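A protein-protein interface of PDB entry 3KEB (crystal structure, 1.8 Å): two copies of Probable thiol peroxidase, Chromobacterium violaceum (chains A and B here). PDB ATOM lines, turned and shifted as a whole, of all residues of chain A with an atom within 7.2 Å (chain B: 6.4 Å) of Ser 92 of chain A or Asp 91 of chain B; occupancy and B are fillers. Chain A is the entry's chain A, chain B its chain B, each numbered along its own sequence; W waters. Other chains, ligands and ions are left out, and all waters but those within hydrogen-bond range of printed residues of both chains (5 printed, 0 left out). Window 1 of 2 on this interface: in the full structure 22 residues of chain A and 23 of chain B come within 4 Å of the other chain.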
ATOM      1  N   VAL A  34      -9.649 -15.485   3.606  1.00  0.00           N
ATOM      2  CA  VAL A  34      -8.987 -14.201   3.726  1.00  0.00           C
ATOM      3  C   VAL A  34      -8.925 -13.561   2.357  1.00  0.00           C
ATOM      4  O   VAL A  34      -8.630 -14.184   1.363  1.00  0.00           O
ATOM      5  CB  VAL A  34      -7.601 -14.319   4.398  1.00  0.00           C
ATOM      6  CG1 VAL A  34      -6.814 -15.367   3.746  1.00  0.00           C
ATOM      7  CG2 VAL A  34      -6.861 -12.983   4.378  1.00  0.00           C
ATOM      8  N   ASP A  35      -9.282 -12.301   2.285  1.00  0.00           N
ATOM      9  CA  ASP A  35      -9.335 -11.606   0.998  1.00  0.00           C
ATOM     10  C   ASP A  35      -8.005 -11.006   0.589  1.00  0.00           C
ATOM     11  O   ASP A  35      -7.020 -11.101   1.300  1.00  0.00           O
ATOM     12  CB  ASP A  35     -10.451 -10.554   1.001  1.00  0.00           C
ATOM     13  CG  ASP A  35     -10.162  -9.329   1.857  1.00  0.00           C
ATOM     14  OD1 ASP A  35      -8.997  -8.955   2.204  1.00  0.00           O
ATOM     15  OD2 ASP A  35     -11.199  -8.637   2.174  1.00  0.00           O
ATOM     16  N   ASP A  36      -7.985 -10.348  -0.560  1.00  0.00           N
ATOM     17  CA  ASP A  36      -6.739  -9.848  -1.097  1.00  0.00           C
ATOM     18  C   ASP A  36      -6.059  -8.731  -0.322  1.00  0.00           C
ATOM     19  O   ASP A  36      -4.844  -8.500  -0.508  1.00  0.00           O
ATOM     20  CB  ASP A  36      -6.867  -9.499  -2.578  1.00  0.00           C
ATOM     21  CG  ASP A  36      -7.850  -8.350  -2.859  1.00  0.00           C
ATOM     22  OD1 ASP A  36      -9.017  -8.427  -2.461  1.00  0.00           O
ATOM     23  OD2 ASP A  36      -7.430  -7.334  -3.458  1.00  0.00           O
ATOM     24  N   VAL A  59      -5.553 -17.439 -10.150  1.00  0.00           N
ATOM     25  CA  VAL A  59      -5.530 -16.197 -10.991  1.00  0.00           C
ATOM     26  C   VAL A  59      -4.270 -16.063 -11.860  1.00  0.00           C
ATOM     27  O   VAL A  59      -4.223 -15.199 -12.766  1.00  0.00           O
ATOM     28  CB  VAL A  59      -5.651 -14.876 -10.141  1.00  0.00           C
ATOM     29  CG1 VAL A  59      -7.000 -14.746  -9.464  1.00  0.00           C
ATOM     30  CG2 VAL A  59      -4.499 -14.730  -9.098  1.00  0.00           C
ATOM     31  N   THR A  89      -9.641 -19.074  -4.415  1.00  0.00           N
ATOM     32  CA  THR A  89      -8.559 -19.901  -4.879  1.00  0.00           C
ATOM     33  C   THR A  89      -7.538 -20.181  -3.797  1.00  0.00           C
ATOM     34  O   THR A  89      -7.589 -19.627  -2.701  1.00  0.00           O
ATOM     35  CB  THR A  89      -7.778 -19.308  -6.086  1.00  0.00           C
ATOM     36  OG1 THR A  89      -6.889 -18.304  -5.616  1.00  0.00           O
ATOM     37  CG2 THR A  89      -8.667 -18.645  -7.181  1.00  0.00           C
ATOM     38  N   VAL A  90      -6.558 -20.993  -4.148  1.00  0.00           N
ATOM     39  CA  VAL A  90      -5.439 -21.313  -3.286  1.00  0.00           C
ATOM     40  C   VAL A  90      -4.332 -20.283  -3.295  1.00  0.00           C
ATOM     41  O   VAL A  90      -3.369 -20.388  -2.518  1.00  0.00           O
ATOM     42  CB  VAL A  90      -4.847 -22.733  -3.634  1.00  0.00           C
ATOM     43  CG1 VAL A  90      -3.841 -22.681  -4.792  1.00  0.00           C
ATOM     44  CG2 VAL A  90      -4.228 -23.346  -2.397  1.00  0.00           C
ATOM     45  N   ASP A  91      -4.458 -19.293  -4.165  1.00  0.00           N
ATOM     46  CA  ASP A  91      -3.459 -18.240  -4.247  1.00  0.00           C
ATOM     47  C   ASP A  91      -3.315 -17.511  -2.926  1.00  0.00           C
ATOM     48  O   ASP A  91      -4.287 -17.409  -2.145  1.00  0.00           O
ATOM     49  CB  ASP A  91      -3.828 -17.218  -5.312  1.00  0.00           C
ATOM     50  CG  ASP A  91      -3.898 -17.808  -6.665  1.00  0.00           C
ATOM     51  OD1 ASP A  91      -2.910 -18.476  -7.073  1.00  0.00           O
ATOM     52  OD2 ASP A  91      -4.924 -17.572  -7.372  1.00  0.00           O
ATOM     53  N   SER A  92      -2.128 -16.971  -2.689  1.00  0.00           N
ATOM     54  CA  SER A  92      -1.910 -16.150  -1.511  1.00  0.00           C
ATOM     55  C   SER A  92      -2.722 -14.835  -1.641  1.00  0.00           C
ATOM     56  O   SER A  92      -2.933 -14.339  -2.760  1.00  0.00           O
ATOM     57  CB  SER A  92      -0.452 -15.791  -1.337  1.00  0.00           C
ATOM     58  OG  SER A  92      -0.017 -14.992  -2.428  1.00  0.00           O
ATOM     59  N   PRO A  93      -3.092 -14.227  -0.493  1.00  0.00           N
ATOM     60  CA  PRO A  93      -3.636 -12.891  -0.589  1.00  0.00           C
ATOM     61  C   PRO A  93      -2.742 -11.928  -1.373  1.00  0.00           C
ATOM     62  O   PRO A  93      -3.250 -11.106  -2.142  1.00  0.00           O
ATOM     63  CB  PRO A  93      -3.776 -12.473   0.857  1.00  0.00           C
ATOM     64  CG  PRO A  93      -3.999 -13.748   1.615  1.00  0.00           C
ATOM     65  CD  PRO A  93      -3.142 -14.771   0.873  1.00  0.00           C
ATOM     66  N   SER A  94      -1.438 -12.000  -1.183  1.00  0.00           N
ATOM     67  CA  SER A  94      -0.507 -11.108  -1.905  1.00  0.00           C
ATOM     68  C   SER A  94      -0.647 -11.246  -3.434  1.00  0.00           C
ATOM     69  O   SER A  94      -0.593 -10.233  -4.176  1.00  0.00           O
ATOM     70  CB  SER A  94       0.947 -11.393  -1.483  1.00  0.00           C
ATOM     71  OG  SER A  94       1.018 -11.424  -0.038  1.00  0.00           O
ATOM     72  N   SER A  95      -0.700 -12.486  -3.916  1.00  0.00           N
ATOM     73  CA  SER A  95      -0.896 -12.728  -5.356  1.00  0.00           C
ATOM     74  C   SER A  95      -2.266 -12.283  -5.858  1.00  0.00           C
ATOM     75  O   SER A  95      -2.370 -11.791  -6.969  1.00  0.00           O
ATOM     76  CB  SER A  95      -0.694 -14.204  -5.715  1.00  0.00           C
ATOM     77  OG  SER A  95       0.614 -14.596  -5.354  1.00  0.00           O
ATOM     78  N   LEU A  96      -3.305 -12.447  -5.040  1.00  0.00           N
ATOM     79  CA  LEU A  96      -4.663 -11.974  -5.400  1.00  0.00           C
ATOM     80  C   LEU A  96      -4.635 -10.425  -5.527  1.00  0.00           C
ATOM     81  O   LEU A  96      -5.184  -9.853  -6.472  1.00  0.00           O
ATOM     82  CB  LEU A  96      -5.683 -12.471  -4.377  1.00  0.00           C
ATOM     83  CG  LEU A  96      -5.929 -13.979  -4.353  1.00  0.00           C
ATOM     84  CD1 LEU A  96      -6.844 -14.409  -3.156  1.00  0.00           C
ATOM     85  CD2 LEU A  96      -6.494 -14.446  -5.692  1.00  0.00           C
ATOM     86  N   ALA A  97      -3.963  -9.751  -4.596  1.00  0.00           N
ATOM     87  CA  ALA A  97      -3.815  -8.305  -4.652  1.00  0.00           C
ATOM     88  C   ALA A  97      -3.067  -7.859  -5.899  1.00  0.00           C
ATOM     89  O   ALA A  97      -3.466  -6.869  -6.567  1.00  0.00           O
ATOM     90  CB  ALA A  97      -3.185  -7.781  -3.374  1.00  0.00           C
ATOM     91  N   ARG A  98      -2.029  -8.599  -6.268  1.00  0.00           N
ATOM     92  CA  ARG A  98      -1.288  -8.311  -7.495  1.00  0.00           C
ATOM     93  C   ARG A  98      -2.206  -8.471  -8.741  1.00  0.00           C
ATOM     94  O   ARG A  98      -2.220  -7.611  -9.601  1.00  0.00           O
ATOM     95  CB  ARG A  98      -0.111  -9.240  -7.656  1.00  0.00           C
ATOM     96  CG  ARG A  98       0.639  -9.011  -8.922  1.00  0.00           C
ATOM     97  CD  ARG A  98       1.088 -10.336  -9.524  1.00  0.00           C
ATOM     98  NE  ARG A  98       1.563 -10.068 -10.878  1.00  0.00           N
ATOM     99  CZ  ARG A  98       0.932 -10.391 -12.008  1.00  0.00           C
ATOM    100  NH1 ARG A  98      -0.237 -11.062 -12.007  1.00  0.00           N
ATOM    101  NH2 ARG A  98       1.515 -10.058 -13.156  1.00  0.00           N
ATOM    102  N   LEU A 111     -10.700 -14.206  -2.733  1.00  0.00           N
ATOM    103  CA  LEU A 111     -10.508 -14.856  -1.446  1.00  0.00           C
ATOM    104  C   LEU A 111      -9.560 -16.017  -1.592  1.00  0.00           C
ATOM    105  O   LEU A 111      -9.660 -16.788  -2.542  1.00  0.00           O
ATOM    106  CB  LEU A 111     -11.838 -15.379  -0.904  1.00  0.00           C
ATOM    107  CG  LEU A 111     -12.997 -14.363  -0.911  1.00  0.00           C
ATOM    108  CD1 LEU A 111     -14.203 -15.006  -0.171  1.00  0.00           C
ATOM    109  CD2 LEU A 111     -12.626 -13.006  -0.274  1.00  0.00           C
ATOM    110  N   SER A 112      -8.701 -16.154  -0.590  1.00  0.00           N
ATOM    111  CA  SER A 112      -7.684 -17.158  -0.511  1.00  0.00           C
ATOM    112  C   SER A 112      -8.059 -18.176   0.555  1.00  0.00           C
ATOM    113  O   SER A 112      -8.619 -17.824   1.628  1.00  0.00           O
ATOM    114  CB  SER A 112      -6.374 -16.517  -0.106  1.00  0.00           C
ATOM    115  OG  SER A 112      -5.432 -17.493   0.252  1.00  0.00           O
ATOM    116  N   THR A 113      -7.734 -19.423   0.275  1.00  0.00           N
ATOM    117  CA  THR A 113      -7.974 -20.489   1.226  1.00  0.00           C
ATOM    118  C   THR A 113      -6.820 -20.688   2.191  1.00  0.00           C
ATOM    119  O   THR A 113      -6.810 -21.677   2.971  1.00  0.00           O
ATOM    120  CB  THR A 113      -8.239 -21.804   0.534  1.00  0.00           C
ATOM    121  OG1 THR A 113      -7.113 -22.183  -0.248  1.00  0.00           O
ATOM    122  CG2 THR A 113      -9.474 -21.691  -0.411  1.00  0.00           C
ATOM    123  N   LEU A 114      -5.844 -19.786   2.204  1.00  0.00           N
ATOM    124  CA  LEU A 114      -4.709 -20.070   3.111  1.00  0.00           C
ATOM    125  C   LEU A 114      -5.116 -20.102   4.604  1.00  0.00           C
ATOM    126  O   LEU A 114      -4.563 -20.865   5.327  1.00  0.00           O
ATOM    127  CB  LEU A 114      -3.480 -19.182   2.842  1.00  0.00           C
ATOM    128  CG  LEU A 114      -3.315 -17.993   3.718  1.00  0.00           C
ATOM    129  CD1 LEU A 114      -2.026 -17.193   3.480  1.00  0.00           C
ATOM    130  CD2 LEU A 114      -4.556 -17.171   3.440  1.00  0.00           C
ATOM    131  N   ARG A 117      -7.457 -24.385   4.758  1.00  0.00           N
ATOM    132  CA  ARG A 117      -7.613 -25.128   3.521  1.00  0.00           C
ATOM    133  C   ARG A 117      -8.795 -26.135   3.571  1.00  0.00           C
ATOM    134  O   ARG A 117      -9.196 -26.626   2.534  1.00  0.00           O
ATOM    135  CB  ARG A 117      -6.307 -25.828   3.168  1.00  0.00           C
ATOM    136  CG  ARG A 117      -5.059 -24.877   3.057  1.00  0.00           C
ATOM    137  CD  ARG A 117      -5.038 -23.977   1.773  1.00  0.00           C
ATOM    138  NE  ARG A 117      -3.672 -23.493   1.505  1.00  0.00           N
ATOM    139  CZ  ARG A 117      -3.330 -22.389   0.826  1.00  0.00           C
ATOM    140  NH1 ARG A 117      -2.041 -22.113   0.643  1.00  0.00           N
ATOM    141  NH2 ARG A 117      -4.259 -21.576   0.306  1.00  0.00           N
ATOM    142  N   LEU B  56       9.822 -16.500   2.483  1.00  0.00           N
ATOM    143  CA  LEU B  56       9.348 -15.136   2.288  1.00  0.00           C
ATOM    144  C   LEU B  56       7.847 -15.127   2.552  1.00  0.00           C
ATOM    145  O   LEU B  56       7.171 -16.172   2.493  1.00  0.00           O
ATOM    146  CB  LEU B  56       9.589 -14.753   0.822  1.00  0.00           C
ATOM    147  CG  LEU B  56      11.034 -14.790   0.396  1.00  0.00           C
ATOM    148  CD1 LEU B  56      11.058 -14.500  -1.138  1.00  0.00           C
ATOM    149  CD2 LEU B  56      11.798 -13.808   1.236  1.00  0.00           C
ATOM    150  N   LEU B  57       7.292 -13.944   2.774  1.00  0.00           N
ATOM    151  CA  LEU B  57       5.836 -13.852   2.845  1.00  0.00           C
ATOM    152  C   LEU B  57       5.232 -14.239   1.481  1.00  0.00           C
ATOM    153  O   LEU B  57       4.310 -15.085   1.401  1.00  0.00           O
ATOM    154  CB  LEU B  57       5.415 -12.446   3.264  1.00  0.00           C
ATOM    155  CG  LEU B  57       5.688 -12.057   4.697  1.00  0.00           C
ATOM    156  CD1 LEU B  57       5.121 -10.695   4.895  1.00  0.00           C
ATOM    157  CD2 LEU B  57       5.005 -13.016   5.716  1.00  0.00           C
ATOM    158  N   SER B  58       5.735 -13.609   0.421  1.00  0.00           N
ATOM    159  CA  SER B  58       5.261 -13.880  -0.920  1.00  0.00           C
ATOM    160  C   SER B  58       6.203 -13.258  -1.918  1.00  0.00           C
ATOM    161  O   SER B  58       6.725 -12.149  -1.698  1.00  0.00           O
ATOM    162  CB  SER B  58       3.875 -13.283  -1.119  1.00  0.00           C
ATOM    163  OG  SER B  58       3.425 -13.444  -2.465  1.00  0.00           O
ATOM    164  N   VAL B  59       6.352 -13.919  -3.051  1.00  0.00           N
ATOM    165  CA  VAL B  59       7.056 -13.309  -4.178  1.00  0.00           C
ATOM    166  C   VAL B  59       6.314 -12.098  -4.717  1.00  0.00           C
ATOM    167  O   VAL B  59       6.913 -11.322  -5.465  1.00  0.00           O
ATOM    168  CB  VAL B  59       7.326 -14.283  -5.317  1.00  0.00           C
ATOM    169  CG1 VAL B  59       8.189 -15.453  -4.872  1.00  0.00           C
ATOM    170  CG2 VAL B  59       5.992 -14.670  -6.085  1.00  0.00           C
ATOM    171  N   ASP B  60       5.032 -11.923  -4.355  1.00  0.00           N
ATOM    172  CA  ASP B  60       4.237 -10.756  -4.783  1.00  0.00           C
ATOM    173  C   ASP B  60       4.128  -9.641  -3.735  1.00  0.00           C
ATOM    174  O   ASP B  60       3.379  -8.691  -3.910  1.00  0.00           O
ATOM    175  CB  ASP B  60       2.848 -11.207  -5.272  1.00  0.00           C
ATOM    176  CG  ASP B  60       2.932 -12.019  -6.564  1.00  0.00           C
ATOM    177  OD1 ASP B  60       3.703 -11.634  -7.495  1.00  0.00           O
ATOM    178  OD2 ASP B  60       2.248 -13.047  -6.695  1.00  0.00           O
ATOM    179  N   THR B  89       7.373 -20.323  -0.085  1.00  0.00           N
ATOM    180  CA  THR B  89       6.273 -19.400   0.296  1.00  0.00           C
ATOM    181  C   THR B  89       4.932 -20.160   0.246  1.00  0.00           C
ATOM    182  O   THR B  89       4.848 -21.313  -0.244  1.00  0.00           O
ATOM    183  CB  THR B  89       6.146 -18.167  -0.651  1.00  0.00           C
ATOM    184  OG1 THR B  89       5.535 -18.590  -1.875  1.00  0.00           O
ATOM    185  CG2 THR B  89       7.527 -17.492  -0.928  1.00  0.00           C
ATOM    186  N   VAL B  90       3.865 -19.500   0.721  1.00  0.00           N
ATOM    187  CA  VAL B  90       2.507 -20.000   0.588  1.00  0.00           C
ATOM    188  C   VAL B  90       1.880 -19.701  -0.768  1.00  0.00           C
ATOM    189  O   VAL B  90       0.724 -20.052  -0.999  1.00  0.00           O
ATOM    190  CB  VAL B  90       1.533 -19.457   1.672  1.00  0.00           C
ATOM    191  CG1 VAL B  90       2.037 -19.856   3.005  1.00  0.00           C
ATOM    192  CG2 VAL B  90       1.323 -17.880   1.473  1.00  0.00           C
ATOM    193  N   ASP B  91       2.600 -19.001  -1.644  1.00  0.00           N
ATOM    194  CA  ASP B  91       2.106 -18.734  -2.962  1.00  0.00           C
ATOM    195  C   ASP B  91       1.793 -20.005  -3.697  1.00  0.00           C
ATOM    196  O   ASP B  91       2.441 -21.009  -3.479  1.00  0.00           O
ATOM    197  CB  ASP B  91       3.114 -17.967  -3.827  1.00  0.00           C
ATOM    198  CG  ASP B  91       3.449 -16.615  -3.267  1.00  0.00           C
ATOM    199  OD1 ASP B  91       2.518 -15.810  -3.000  1.00  0.00           O
ATOM    200  OD2 ASP B  91       4.682 -16.412  -3.011  1.00  0.00           O
ATOM    201  N   SER B  92       0.854 -19.937  -4.640  1.00  0.00           N
ATOM    202  CA  SER B  92       0.561 -21.100  -5.499  1.00  0.00           C
ATOM    203  C   SER B  92       1.711 -21.393  -6.465  1.00  0.00           C
ATOM    204  O   SER B  92       2.454 -20.489  -6.820  1.00  0.00           O
ATOM    205  CB  SER B  92      -0.726 -20.890  -6.308  1.00  0.00           C
ATOM    206  OG  SER B  92      -0.557 -19.842  -7.281  1.00  0.00           O
ATOM    207  N   PRO B  93       1.852 -22.651  -6.914  1.00  0.00           N
ATOM    208  CA  PRO B  93       2.800 -22.920  -8.014  1.00  0.00           C
ATOM    209  C   PRO B  93       2.568 -22.058  -9.214  1.00  0.00           C
ATOM    210  O   PRO B  93       3.523 -21.574  -9.803  1.00  0.00           O
ATOM    211  CB  PRO B  93       2.539 -24.391  -8.345  1.00  0.00           C
ATOM    212  CG  PRO B  93       2.108 -24.983  -7.018  1.00  0.00           C
ATOM    213  CD  PRO B  93       1.255 -23.879  -6.390  1.00  0.00           C
ATOM    214  N   SER B  94       1.294 -21.809  -9.530  1.00  0.00           N
ATOM    215  CA  SER B  94       0.912 -21.015 -10.657  1.00  0.00           C
ATOM    216  C   SER B  94       1.477 -19.577 -10.499  1.00  0.00           C
ATOM    217  O   SER B  94       2.120 -19.042 -11.419  1.00  0.00           O
ATOM    218  CB  SER B  94      -0.616 -21.012 -10.821  1.00  0.00           C
ATOM    219  OG  SER B  94      -1.174 -22.329 -10.880  1.00  0.00           O
ATOM    220  N   SER B  95       1.315 -18.983  -9.333  1.00  0.00           N
ATOM    221  CA  SER B  95       1.848 -17.621  -9.080  1.00  0.00           C
ATOM    222  C   SER B  95       3.373 -17.591  -9.073  1.00  0.00           C
ATOM    223  O   SER B  95       3.981 -16.664  -9.577  1.00  0.00           O
ATOM    224  CB  SER B  95       1.291 -17.039  -7.800  1.00  0.00           C
ATOM    225  OG  SER B  95      -0.125 -17.090  -7.831  1.00  0.00           O
ATOM    226  N   LEU B  96       3.975 -18.623  -8.523  1.00  0.00           N
ATOM    227  CA  LEU B  96       5.439 -18.757  -8.536  1.00  0.00           C
ATOM    228  C   LEU B  96       5.979 -18.852  -9.947  1.00  0.00           C
ATOM    229  O   LEU B  96       6.966 -18.170 -10.233  1.00  0.00           O
ATOM    230  CB  LEU B  96       5.896 -19.950  -7.693  1.00  0.00           C
ATOM    231  CG  LEU B  96       5.672 -19.893  -6.161  1.00  0.00           C
ATOM    232  CD1 LEU B  96       6.047 -21.201  -5.421  1.00  0.00           C
ATOM    233  CD2 LEU B  96       6.416 -18.687  -5.501  1.00  0.00           C
ATOM    234  N   LEU B 111       9.336 -22.947  -4.269  1.00  0.00           N
ATOM    235  CA  LEU B 111       8.514 -24.019  -3.723  1.00  0.00           C
ATOM    236  C   LEU B 111       7.323 -23.426  -2.986  1.00  0.00           C
ATOM    237  O   LEU B 111       7.468 -22.463  -2.235  1.00  0.00           O
ATOM    238  CB  LEU B 111       9.328 -24.902  -2.751  1.00  0.00           C
ATOM    239  CG  LEU B 111      10.626 -25.499  -3.271  1.00  0.00           C
ATOM    240  CD1 LEU B 111      11.367 -26.456  -2.189  1.00  0.00           C
ATOM    241  CD2 LEU B 111      10.461 -26.195  -4.631  1.00  0.00           C
ATOM    242  N   SER B 112       6.164 -23.980  -3.246  1.00  0.00           N
ATOM    243  CA  SER B 112       4.939 -23.630  -2.610  1.00  0.00           C
ATOM    244  C   SER B 112       4.632 -24.609  -1.444  1.00  0.00           C
ATOM    245  O   SER B 112       4.747 -25.817  -1.605  1.00  0.00           O
ATOM    246  CB  SER B 112       3.825 -23.815  -3.554  1.00  0.00           C
ATOM    247  OG  SER B 112       2.567 -23.701  -2.886  1.00  0.00           O
ATOM    248  N   THR B 113       4.061 -24.098  -0.355  1.00  0.00           N
ATOM    249  CA  THR B 113       3.596 -24.965   0.744  1.00  0.00           C
ATOM    250  C   THR B 113       2.123 -25.405   0.611  1.00  0.00           C
ATOM    251  O   THR B 113       1.535 -25.917   1.576  1.00  0.00           O
ATOM    252  CB  THR B 113       3.698 -24.245   2.099  1.00  0.00           C
ATOM    253  OG1 THR B 113       2.852 -23.083   2.087  1.00  0.00           O
ATOM    254  CG2 THR B 113       5.092 -23.764   2.355  1.00  0.00           C
ATOM    255  N   LEU B 114       1.503 -25.252  -0.561  1.00  0.00           N
ATOM    256  CA  LEU B 114       0.032 -25.444  -0.591  1.00  0.00           C
ATOM    257  C   LEU B 114      -0.533 -26.790  -0.097  1.00  0.00           C
ATOM    258  O   LEU B 114      -1.701 -26.833   0.342  1.00  0.00           O
ATOM    259  CB  LEU B 114      -0.542 -25.096  -1.970  1.00  0.00           C
ATOM    260  CG  LEU B 114      -0.512 -26.188  -3.000  1.00  0.00           C
ATOM    261  CD1 LEU B 114      -1.313 -25.773  -4.251  1.00  0.00           C
ATOM    262  CD2 LEU B 114       0.939 -26.489  -3.352  1.00  0.00           C
ATOM    263  N   TYR B 135       0.682 -17.492   6.561  1.00  0.00           N
ATOM    264  CA  TYR B 135       1.932 -17.204   5.871  1.00  0.00           C
ATOM    265  C   TYR B 135       3.121 -17.857   6.532  1.00  0.00           C
ATOM    266  O   TYR B 135       3.091 -18.137   7.715  1.00  0.00           O
ATOM    267  CB  TYR B 135       2.225 -15.721   5.843  1.00  0.00           C
ATOM    268  CG  TYR B 135       1.498 -14.954   4.789  1.00  0.00           C
ATOM    269  CD1 TYR B 135       2.117 -14.621   3.614  1.00  0.00           C
ATOM    270  CD2 TYR B 135       0.183 -14.553   4.975  1.00  0.00           C
ATOM    271  CE1 TYR B 135       1.485 -13.910   2.611  1.00  0.00           C
ATOM    272  CE2 TYR B 135      -0.473 -13.814   3.952  1.00  0.00           C
ATOM    273  CZ  TYR B 135       0.204 -13.515   2.793  1.00  0.00           C
ATOM    274  OH  TYR B 135      -0.417 -12.815   1.789  1.00  0.00           O
HETATM  275  O   HOH W   1       0.753  -7.947  -3.681  1.00  0.00           O
HETATM  276  O   HOH W   2      -0.267 -17.255  -5.029  1.00  0.00           O
HETATM  277  O   HOH W   3      -0.224 -23.191   2.688  1.00  0.00           O
HETATM  278  O   HOH W   4      -0.957 -21.862  -2.368  1.00  0.00           O
HETATM  279  O   HOH W   5      -1.929 -19.370  -0.323  1.00  0.00           O
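The side-chain hydroxyl of Ser 95 of chain A is in hydrogen-bond range of the side-chain carboxylate of Asp 60 of chain B, at 2.6 Å.
The side-chain carboxylate (OD1) of Asp 91 of chain B lies within hydrogen-bond range of the side-chain hydroxyl (OG) of Ser 95 of chain A (3.3 Å).
OG of Ser 95 of chain B sits at hydrogen-bond distance from OD1 of Asp 91 of chain A.
OG of Ser 94 of chain A lies within hydrogen-bond range of OH of Tyr 135 of chain B, 2.7 Å away.
OD1 of Asp 91 of chain B lies within hydrogen-bond range of OG of Ser 92 of chain A (2.7 Å).
OG of Ser 92 of chain B is in hydrogen-bond range of OD1 of Asp 91 of chain A.
OG of Ser 58 of chain B sits at hydrogen-bond distance from OD1 of Asp 91 of chain B.
OG of Ser 58 of chain B is in hydrogen-bond range of N of Asp 60 of chain B.
The backbone NH of Val 59 of chain A lies within hydrogen-bond range of the side-chain carboxylate of Asp 91 of chain A, at 2.9 Å.
OG of Ser 112 of chain B is in hydrogen-bond range of O of Asp 91 of chain B, at 2.8 Å.
The backbone NH (N) of Ser 95 of chain A is in hydrogen-bond range of the side-chain hydroxyl (OG) of Ser 92 of chain A, 3.0 Å away.
The side-chain hydroxyl (OG) of Ser 92 of chain B is in hydrogen-bond range of the side-chain hydroxyl (OG) of Ser 95 of chain B (2.8 Å).
CG1 of Val 90 of chain A touches CB of Ser 92 of chain B, 3.9 Å away.
OG of Ser 92 of chain A touches OG of Ser 58 of chain B, at 3.8 Å.
CD of Pro 93 of chain A touches OH of Tyr 135 of chain B, at 3.5 Å.
Ser 94 of chain A touches Ser 58 of chain B.
Ser 94 of chain A touches Asp 60 of chain B.
Ser 95 of chain A touches Ser 95 of chain B (OG to CB, 3.5 Å).
Arg 98 of chain A touches Asp 60 of chain B (CD to OD1, 3.6 Å).
Val 90 of chain B touches Leu 114 of chain A (CG2 to CD1, 3.96 Å).
Leu 114 of chain A touches Tyr 135 of chain B.
NH1 of Arg 117 of chain A touches O of Val 90 of chain B (3.8 Å).
Printed residues of chain B within 4 Å of Val 90 of chain A: Ser 92 (3.9 Å).
Of the printed residues of chain B, Leu 114 of chain A touches Val 90 and Tyr 135.
Of the printed residues of chain B, Arg 117 of chain A touches Val 90 (3.8 Å).
Val 59 of chain B touches none of the printed residues of chain A.
Of chain A, only Ser 92 (2.7 Å) and Ser 95 (3.3 Å) come within 4 Å of Asp 91 of chain B.
Printed residues of chain A within 4 Å of Ser 92 of chain B: Val 90 and Asp 91.
Of the printed residues of chain A, Ser 95 of chain B touches Asp 91 (3.2 Å) and Ser 95 (3.5 Å).
The nearest residue of chain B that does not touch Ser 92 of chain A is Tyr 135 of chain B (4.3 Å).
Hydrophobic or aromatic side chains of chain A within 4 Å of the printed part of chain B: Val 90, Pro 93 and Leu 114.
Along chain A the printed residues that touch a printed residue of chain B span positions 90 to 117.
Of the 18 printed residues of chain B, 7 touch a printed residue of chain A.
Hydrophobic or aromatic side chains of chain B within 4 Å of the printed part of chain A: Val 90 and Tyr 135.
Along chain B the printed residues that touch a printed residue of chain A span positions 58 to 135.
Among the printed residues, no Asp or Glu carboxylate lies within 4 Å of a Lys or Arg side-chain nitrogen of the other chain.
Val 90 of chain A touches Ser 92 of chain B, and with the chains exchanged Ser 92 of chain A touches Val 90 of chain B.
Asp 91 of chain A touches Ser 95 of chain B, and with the chains exchanged Ser 95 of chain A touches Asp 91 of chain B.
Ser 95 of chain A touches its own counterpart, Ser 95 of chain B.
Leu 114 of chain A touches Val 90 of chain B, but with the chains exchanged Val 90 of chain A does not touch Leu 114 of chain B (4.03 Å).
Of the 17 pairs that touch across the chains among the printed residues, 7 have their exchanged pair printed and touching as well.
Water W1 lies within hydrogen-bond range of the backbone carbonyl oxygen of Ser 94 of chain A (2.7 Å) and the backbone carbonyl oxygen of Asp 60 of chain B (2.7 Å).
Water W2 lies within hydrogen-bond range of the side-chain hydroxyl of Ser 95 of chain B, the side-chain hydroxyl of Ser 95 of chain A, the backbone NH of Ser 92 of chain B and the backbone NH of Ser 92 of chain A.
Water W5 lies within hydrogen-bond range of O of Val 90 of chain A (2.8 Å), O of Val 90 of chain B (2.8 Å), NH1 of Arg 117 of chain A (2.9 Å) and N of Ser 92 of chain A (3.4 Å).
Water W4 lies within hydrogen-bond range of O of Val 90 of chain B, O of Val 90 of chain A, NH1 of Arg 117 of chain A and N of Ser 92 of chain B.
Water W3 lies within hydrogen-bond range of the guanidinium group of Arg 117 of chain A (2.9 Å) and the side-chain hydroxyl of Thr 113 of chain B (3.1 Å).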
